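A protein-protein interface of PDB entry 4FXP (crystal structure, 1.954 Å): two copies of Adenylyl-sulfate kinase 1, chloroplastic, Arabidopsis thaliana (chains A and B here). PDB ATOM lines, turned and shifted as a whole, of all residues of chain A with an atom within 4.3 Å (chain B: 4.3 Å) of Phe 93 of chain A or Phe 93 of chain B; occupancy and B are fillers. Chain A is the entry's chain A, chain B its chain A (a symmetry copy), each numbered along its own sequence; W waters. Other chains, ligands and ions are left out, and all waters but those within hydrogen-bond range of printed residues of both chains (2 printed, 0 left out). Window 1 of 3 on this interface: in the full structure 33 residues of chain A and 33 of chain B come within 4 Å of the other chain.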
ATOM      1  N   TYR A  57      23.518  11.928 -20.819  1.00  0.00           N
ATOM      2  CA  TYR A  57      23.121  11.041 -21.909  1.00  0.00           C
ATOM      3  C   TYR A  57      23.984   9.789 -21.931  1.00  0.00           C
ATOM      4  O   TYR A  57      25.205   9.875 -21.876  1.00  0.00           O
ATOM      5  CB  TYR A  57      23.174  11.749 -23.273  1.00  0.00           C
ATOM      6  CG  TYR A  57      22.463  10.942 -24.345  1.00  0.00           C
ATOM      7  CD1 TYR A  57      21.068  10.899 -24.400  1.00  0.00           C
ATOM      8  CD2 TYR A  57      23.177  10.211 -25.282  1.00  0.00           C
ATOM      9  CE1 TYR A  57      20.405  10.156 -25.375  1.00  0.00           C
ATOM     10  CE2 TYR A  57      22.530   9.464 -26.250  1.00  0.00           C
ATOM     11  CZ  TYR A  57      21.144   9.447 -26.293  1.00  0.00           C
ATOM     12  OH  TYR A  57      20.497   8.705 -27.250  1.00  0.00           O
ATOM     13  N   VAL A  89      32.471  10.426 -30.065  1.00  0.00           N
ATOM     14  CA  VAL A  89      31.106  10.901 -29.844  1.00  0.00           C
ATOM     15  C   VAL A  89      30.942  11.462 -28.432  1.00  0.00           C
ATOM     16  O   VAL A  89      30.326  12.503 -28.227  1.00  0.00           O
ATOM     17  CB  VAL A  89      30.056   9.809 -30.132  1.00  0.00           C
ATOM     18  CG1 VAL A  89      28.658  10.286 -29.725  1.00  0.00           C
ATOM     19  CG2 VAL A  89      30.079   9.440 -31.614  1.00  0.00           C
ATOM     20  N   ALA A  90      31.523  10.780 -27.455  1.00  0.00           N
ATOM     21  CA  ALA A  90      31.421  11.231 -26.071  1.00  0.00           C
ATOM     22  C   ALA A  90      32.082  12.603 -25.887  1.00  0.00           C
ATOM     23  O   ALA A  90      31.586  13.441 -25.139  1.00  0.00           O
ATOM     24  CB  ALA A  90      32.045  10.178 -25.116  1.00  0.00           C
ATOM     25  N   LYS A  91      33.203  12.823 -26.573  1.00  0.00           N
ATOM     26  CA  LYS A  91      33.863  14.126 -26.579  1.00  0.00           C
ATOM     27  C   LYS A  91      32.940  15.231 -27.106  1.00  0.00           C
ATOM     28  O   LYS A  91      32.922  16.349 -26.581  1.00  0.00           O
ATOM     29  CB  LYS A  91      35.141  14.064 -27.423  1.00  0.00           C
ATOM     30  CG  LYS A  91      35.889  15.376 -27.524  1.00  0.00           C
ATOM     31  CD  LYS A  91      37.122  15.207 -28.377  1.00  0.00           C
ATOM     32  CE  LYS A  91      37.934  16.491 -28.447  1.00  0.00           C
ATOM     33  NZ  LYS A  91      39.246  16.263 -29.115  1.00  0.00           N
ATOM     34  N   LEU A  92      32.184  14.922 -28.155  1.00  0.00           N
ATOM     35  CA  LEU A  92      31.243  15.891 -28.710  1.00  0.00           C
ATOM     36  C   LEU A  92      30.152  16.208 -27.686  1.00  0.00           C
ATOM     37  O   LEU A  92      29.815  17.371 -27.461  1.00  0.00           O
ATOM     38  CB  LEU A  92      30.615  15.364 -30.008  1.00  0.00           C
ATOM     39  CG  LEU A  92      31.537  15.223 -31.230  1.00  0.00           C
ATOM     40  CD1 LEU A  92      30.824  14.527 -32.405  1.00  0.00           C
ATOM     41  CD2 LEU A  92      32.087  16.575 -31.660  1.00  0.00           C
ATOM     42  N   PHE A  93      29.608  15.172 -27.054  1.00  0.00           N
ATOM     43  CA  PHE A  93      28.605  15.388 -26.010  1.00  0.00           C
ATOM     44  C   PHE A  93      29.151  16.244 -24.883  1.00  0.00           C
ATOM     45  O   PHE A  93      28.475  17.150 -24.388  1.00  0.00           O
ATOM     46  CB  PHE A  93      28.047  14.064 -25.477  1.00  0.00           C
ATOM     47  CG  PHE A  93      26.866  13.557 -26.271  1.00  0.00           C
ATOM     48  CD1 PHE A  93      25.583  13.958 -25.952  1.00  0.00           C
ATOM     49  CD2 PHE A  93      27.045  12.707 -27.343  1.00  0.00           C
ATOM     50  CE1 PHE A  93      24.493  13.517 -26.686  1.00  0.00           C
ATOM     51  CE2 PHE A  93      25.957  12.260 -28.082  1.00  0.00           C
ATOM     52  CZ  PHE A  93      24.681  12.672 -27.751  1.00  0.00           C
ATOM     53  N   ALA A  94      30.388  15.971 -24.486  1.00  0.00           N
ATOM     54  CA  ALA A  94      31.008  16.759 -23.431  1.00  0.00           C
ATOM     55  C   ALA A  94      31.162  18.205 -23.881  1.00  0.00           C
ATOM     56  O   ALA A  94      30.962  19.138 -23.097  1.00  0.00           O
ATOM     57  CB  ALA A  94      32.362  16.172 -23.038  1.00  0.00           C
ATOM     58  N   ASP A  95      31.514  18.394 -25.152  1.00  0.00           N
ATOM     59  CA  ASP A  95      31.707  19.742 -25.666  1.00  0.00           C
ATOM     60  C   ASP A  95      30.368  20.480 -25.683  1.00  0.00           C
ATOM     61  O   ASP A  95      30.317  21.706 -25.552  1.00  0.00           O
ATOM     62  CB  ASP A  95      32.325  19.697 -27.068  1.00  0.00           C
ATOM     63  CG  ASP A  95      32.649  21.078 -27.606  1.00  0.00           C
ATOM     64  OD1 ASP A  95      33.184  21.902 -26.839  1.00  0.00           O
ATOM     65  OD2 ASP A  95      32.375  21.327 -28.800  1.00  0.00           O
ATOM     66  N   ALA A  96      29.284  19.724 -25.831  1.00  0.00           N
ATOM     67  CA  ALA A  96      27.932  20.290 -25.828  1.00  0.00           C
ATOM     68  C   ALA A  96      27.482  20.651 -24.410  1.00  0.00           C
ATOM     69  O   ALA A  96      26.428  21.266 -24.230  1.00  0.00           O
ATOM     70  CB  ALA A  96      26.940  19.315 -26.473  1.00  0.00           C
ATOM     71  N   GLY A  97      28.276  20.264 -23.410  1.00  0.00           N
ATOM     72  CA  GLY A  97      27.965  20.544 -22.013  1.00  0.00           C
ATOM     73  C   GLY A  97      27.263  19.407 -21.280  1.00  0.00           C
ATOM     74  O   GLY A  97      26.925  19.519 -20.098  1.00  0.00           O
ATOM     75  N   ILE A  98      27.047  18.298 -21.981  1.00  0.00           N
ATOM     76  CA  ILE A  98      26.341  17.148 -21.416  1.00  0.00           C
ATOM     77  C   ILE A  98      27.258  16.246 -20.583  1.00  0.00           C
ATOM     78  O   ILE A  98      28.431  16.062 -20.916  1.00  0.00           O
ATOM     79  CB  ILE A  98      25.687  16.312 -22.538  1.00  0.00           C
ATOM     80  CG1 ILE A  98      24.644  17.156 -23.278  1.00  0.00           C
ATOM     81  CG2 ILE A  98      25.073  15.018 -21.980  1.00  0.00           C
ATOM     82  CD1 ILE A  98      24.154  16.546 -24.585  1.00  0.00           C
ATOM     83  N   CYS A 100      28.178  12.968 -20.263  1.00  0.00           N
ATOM     84  CA  CYS A 100      28.007  11.812 -21.136  1.00  0.00           C
ATOM     85  C   CYS A 100      28.504  10.536 -20.477  1.00  0.00           C
ATOM     86  O   CYS A 100      29.687  10.448 -20.117  1.00  0.00           O
ATOM     87  CB  CYS A 100      28.762  12.034 -22.449  1.00  0.00           C
ATOM     88  SG  CYS A 100      28.546  10.688 -23.624  1.00  0.00           S
ATOM     89  N   TYR B  57      23.713  22.282 -30.832  1.00  0.00           N
ATOM     90  CA  TYR B  57      25.094  21.868 -31.067  1.00  0.00           C
ATOM     91  C   TYR B  57      25.347  21.645 -32.549  1.00  0.00           C
ATOM     92  O   TYR B  57      24.579  20.961 -33.215  1.00  0.00           O
ATOM     93  CB  TYR B  57      25.459  20.608 -30.268  1.00  0.00           C
ATOM     94  CG  TYR B  57      26.960  20.371 -30.259  1.00  0.00           C
ATOM     95  CD1 TYR B  57      27.801  21.146 -29.457  1.00  0.00           C
ATOM     96  CD2 TYR B  57      27.535  19.397 -31.061  1.00  0.00           C
ATOM     97  CE1 TYR B  57      29.179  20.942 -29.447  1.00  0.00           C
ATOM     98  CE2 TYR B  57      28.903  19.190 -31.064  1.00  0.00           C
ATOM     99  CZ  TYR B  57      29.717  19.964 -30.250  1.00  0.00           C
ATOM    100  OH  TYR B  57      31.075  19.765 -30.252  1.00  0.00           O
ATOM    101  N   VAL B  89      25.012  10.228 -35.405  1.00  0.00           N
ATOM    102  CA  VAL B  89      25.373  11.081 -34.272  1.00  0.00           C
ATOM    103  C   VAL B  89      24.307  12.146 -34.026  1.00  0.00           C
ATOM    104  O   VAL B  89      23.929  12.420 -32.892  1.00  0.00           O
ATOM    105  CB  VAL B  89      26.766  11.719 -34.447  1.00  0.00           C
ATOM    106  CG1 VAL B  89      27.035  12.736 -33.332  1.00  0.00           C
ATOM    107  CG2 VAL B  89      27.843  10.635 -34.446  1.00  0.00           C
ATOM    108  N   ALA B  90      23.798  12.733 -35.101  1.00  0.00           N
ATOM    109  CA  ALA B  90      22.777  13.767 -34.971  1.00  0.00           C
ATOM    110  C   ALA B  90      21.503  13.206 -34.328  1.00  0.00           C
ATOM    111  O   ALA B  90      20.855  13.882 -33.533  1.00  0.00           O
ATOM    112  CB  ALA B  90      22.473  14.398 -36.356  1.00  0.00           C
ATOM    113  N   LYS B  91      21.151  11.970 -34.678  1.00  0.00           N
ATOM    114  CA  LYS B  91      20.028  11.278 -34.048  1.00  0.00           C
ATOM    115  C   LYS B  91      20.218  11.142 -32.533  1.00  0.00           C
ATOM    116  O   LYS B  91      19.270  11.301 -31.757  1.00  0.00           O
ATOM    117  CB  LYS B  91      19.845   9.893 -34.679  1.00  0.00           C
ATOM    118  CG  LYS B  91      18.723   9.074 -34.077  1.00  0.00           C
ATOM    119  CD  LYS B  91      18.632   7.733 -34.763  1.00  0.00           C
ATOM    120  CE  LYS B  91      17.474   6.907 -34.225  1.00  0.00           C
ATOM    121  NZ  LYS B  91      17.263   5.680 -35.042  1.00  0.00           N
ATOM    122  N   LEU B  92      21.441  10.833 -32.114  1.00  0.00           N
ATOM    123  CA  LEU B  92      21.736  10.718 -30.688  1.00  0.00           C
ATOM    124  C   LEU B  92      21.561  12.076 -30.006  1.00  0.00           C
ATOM    125  O   LEU B  92      20.944  12.174 -28.945  1.00  0.00           O
ATOM    126  CB  LEU B  92      23.161  10.192 -30.464  1.00  0.00           C
ATOM    127  CG  LEU B  92      23.447   8.737 -30.870  1.00  0.00           C
ATOM    128  CD1 LEU B  92      24.944   8.396 -30.753  1.00  0.00           C
ATOM    129  CD2 LEU B  92      22.608   7.766 -30.051  1.00  0.00           C
ATOM    130  N   PHE B  93      22.094  13.127 -30.622  1.00  0.00           N
ATOM    131  CA  PHE B  93      21.915  14.473 -30.074  1.00  0.00           C
ATOM    132  C   PHE B  93      20.447  14.836 -29.959  1.00  0.00           C
ATOM    133  O   PHE B  93      20.010  15.402 -28.954  1.00  0.00           O
ATOM    134  CB  PHE B  93      22.681  15.522 -30.887  1.00  0.00           C
ATOM    135  CG  PHE B  93      24.108  15.705 -30.424  1.00  0.00           C
ATOM    136  CD1 PHE B  93      24.407  16.603 -29.418  1.00  0.00           C
ATOM    137  CD2 PHE B  93      25.132  14.963 -30.975  1.00  0.00           C
ATOM    138  CE1 PHE B  93      25.709  16.765 -28.969  1.00  0.00           C
ATOM    139  CE2 PHE B  93      26.439  15.121 -30.531  1.00  0.00           C
ATOM    140  CZ  PHE B  93      26.722  16.022 -29.523  1.00  0.00           C
ATOM    141  N   ALA B  94      19.676  14.493 -30.983  1.00  0.00           N
ATOM    142  CA  ALA B  94      18.248  14.773 -30.950  1.00  0.00           C
ATOM    143  C   ALA B  94      17.590  13.994 -29.819  1.00  0.00           C
ATOM    144  O   ALA B  94      16.699  14.505 -29.133  1.00  0.00           O
ATOM    145  CB  ALA B  94      17.595  14.433 -32.288  1.00  0.00           C
ATOM    146  N   ASP B  95      18.033  12.754 -29.620  1.00  0.00           N
ATOM    147  CA  ASP B  95      17.447  11.925 -28.577  1.00  0.00           C
ATOM    148  C   ASP B  95      17.782  12.515 -27.206  1.00  0.00           C
ATOM    149  O   ASP B  95      17.023  12.360 -26.246  1.00  0.00           O
ATOM    150  CB  ASP B  95      17.954  10.484 -28.691  1.00  0.00           C
ATOM    151  CG  ASP B  95      17.290   9.552 -27.694  1.00  0.00           C
ATOM    152  OD1 ASP B  95      16.059   9.649 -27.523  1.00  0.00           O
ATOM    153  OD2 ASP B  95      18.005   8.720 -27.095  1.00  0.00           O
ATOM    154  N   ALA B  96      18.917  13.204 -27.126  1.00  0.00           N
ATOM    155  CA  ALA B  96      19.347  13.857 -25.886  1.00  0.00           C
ATOM    156  C   ALA B  96      18.553  15.141 -25.628  1.00  0.00           C
ATOM    157  O   ALA B  96      18.683  15.748 -24.562  1.00  0.00           O
ATOM    158  CB  ALA B  96      20.850  14.156 -25.931  1.00  0.00           C
ATOM    159  N   GLY B  97      17.741  15.552 -26.604  1.00  0.00           N
ATOM    160  CA  GLY B  97      16.929  16.757 -26.487  1.00  0.00           C
ATOM    161  C   GLY B  97      17.549  18.003 -27.109  1.00  0.00           C
ATOM    162  O   GLY B  97      16.975  19.095 -27.063  1.00  0.00           O
ATOM    163  N   ILE B  98      18.726  17.839 -27.704  1.00  0.00           N
ATOM    164  CA  ILE B  98      19.456  18.959 -28.301  1.00  0.00           C
ATOM    165  C   ILE B  98      18.971  19.290 -29.716  1.00  0.00           C
ATOM    166  O   ILE B  98      18.615  18.394 -30.485  1.00  0.00           O
ATOM    167  CB  ILE B  98      20.970  18.658 -28.339  1.00  0.00           C
ATOM    168  CG1 ILE B  98      21.504  18.487 -26.913  1.00  0.00           C
ATOM    169  CG2 ILE B  98      21.735  19.752 -29.100  1.00  0.00           C
ATOM    170  CD1 ILE B  98      22.905  17.893 -26.833  1.00  0.00           C
ATOM    171  N   CYS B 100      20.164  19.774 -32.884  1.00  0.00           N
ATOM    172  CA  CYS B 100      21.445  19.462 -33.508  1.00  0.00           C
ATOM    173  C   CYS B 100      21.515  19.987 -34.932  1.00  0.00           C
ATOM    174  O   CYS B 100      20.690  19.603 -35.774  1.00  0.00           O
ATOM    175  CB  CYS B 100      21.667  17.947 -33.513  1.00  0.00           C
ATOM    176  SG  CYS B 100      23.263  17.470 -34.196  1.00  0.00           S
HETATM  177  O   HOH W   1      19.578   6.102 -28.297  1.00  0.00           O
HETATM  178  O   HOH W   2      33.718  20.090 -31.528  1.00  0.00           O
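OD2 of Asp 95 of chain A lies within hydrogen-bond range of OH of Tyr 57 of chain B (2.5 Å). OH of Tyr 57 of chain A sits at hydrogen-bond distance from OD2 of Asp 95 of chain B (2.5 Å).
The backbone carbonyl oxygen of Phe 93 of chain A sits at hydrogen-bond distance from the backbone NH of Ile 98 of chain A. The backbone carbonyl oxygen (O) of Phe 93 of chain B is in hydrogen-bond range of the backbone NH (N) of Ile 98 of chain B, at 3.0 Å.
Tyr 57 of chain A touches Leu 92 of chain B. CB of Ala 96 of chain B touches CD1 of Tyr 57 of chain A (3.6 Å). CG2 of Val 89 of chain A touches CG2 of Val 89 of chain B (3.8 Å). C of Leu 92 of chain A touches CZ of Phe 93 of chain B (3.9 Å). Leu 92 of chain B touches Phe 93 of chain A (C to CZ, 3.9 Å). CE2 of Phe 93 of chain A touches CE2 of Phe 93 of chain B, at 3.8 Å. Phe 93 of chain A touches Ala 96 of chain B (CE1 to CB, 3.8 Å). CB of Ala 96 of chain A touches CD1 of Tyr 57 of chain B, at 3.6 Å. Ala 96 of chain A touches Phe 93 of chain B. Ile 98 of chain B touches Ile 98 of chain A (CD1 to CD1, 2.9 Å).
Of chain B, only Leu 92 (3.9 Å), Phe 93 (3.8 Å) and Ala 96 (3.8 Å) come within 4 Å of Phe 93 of chain A. Of the printed residues of chain B, Asp 95 of chain A touches Tyr 57. Of the printed residues of chain B, Ala 96 of chain A touches Tyr 57 and Phe 93. Lys 91 of chain B touches none of the printed residues of chain A. Of the printed residues of chain A, Ala 96 of chain B touches Tyr 57 and Phe 93. The nearest printed residue of chain B that does not touch Phe 93 of chain A is Ile 98 of chain B (4.7 Å).
Of the 12 printed residues of chain B, 7 touch a printed residue of chain A. Of the 12 printed residues of chain A, 7 touch a printed residue of chain B. Among the printed residues, 13 pairs touch across the chains. Among the printed residues, no Asp or Glu carboxylate lies within 4 Å of a Lys or Arg side-chain nitrogen of the other chain.
Tyr 57 of chain A touches Leu 92 of chain B, and with the chains exchanged Leu 92 of chain A touches Tyr 57 of chain B. Tyr 57 of chain A touches Asp 95 of chain B, and with the chains exchanged Asp 95 of chain A touches Tyr 57 of chain B. Tyr 57 of chain A touches Ala 96 of chain B, and with the chains exchanged Ala 96 of chain A touches Tyr 57 of chain B. Phe 93 of chain A touches Ala 96 of chain B, and with the chains exchanged Ala 96 of chain A touches Phe 93 of chain B. Positions printed for both chains: 57, 89, 90, 91, 92, 93, 94, 95, 96, 97, 98 and 100.
Water W1 bridges the side-chain hydroxyl of Tyr 57 of chain A and the side-chain carboxylate of Asp 95 of chain B. Water W2 lies within hydrogen-bond range of the side-chain hydroxyl (OH) of Tyr 57 of chain B (3.0 Å) and the side-chain carboxylate (OD2) of Asp 95 of chain A (3.3 Å).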
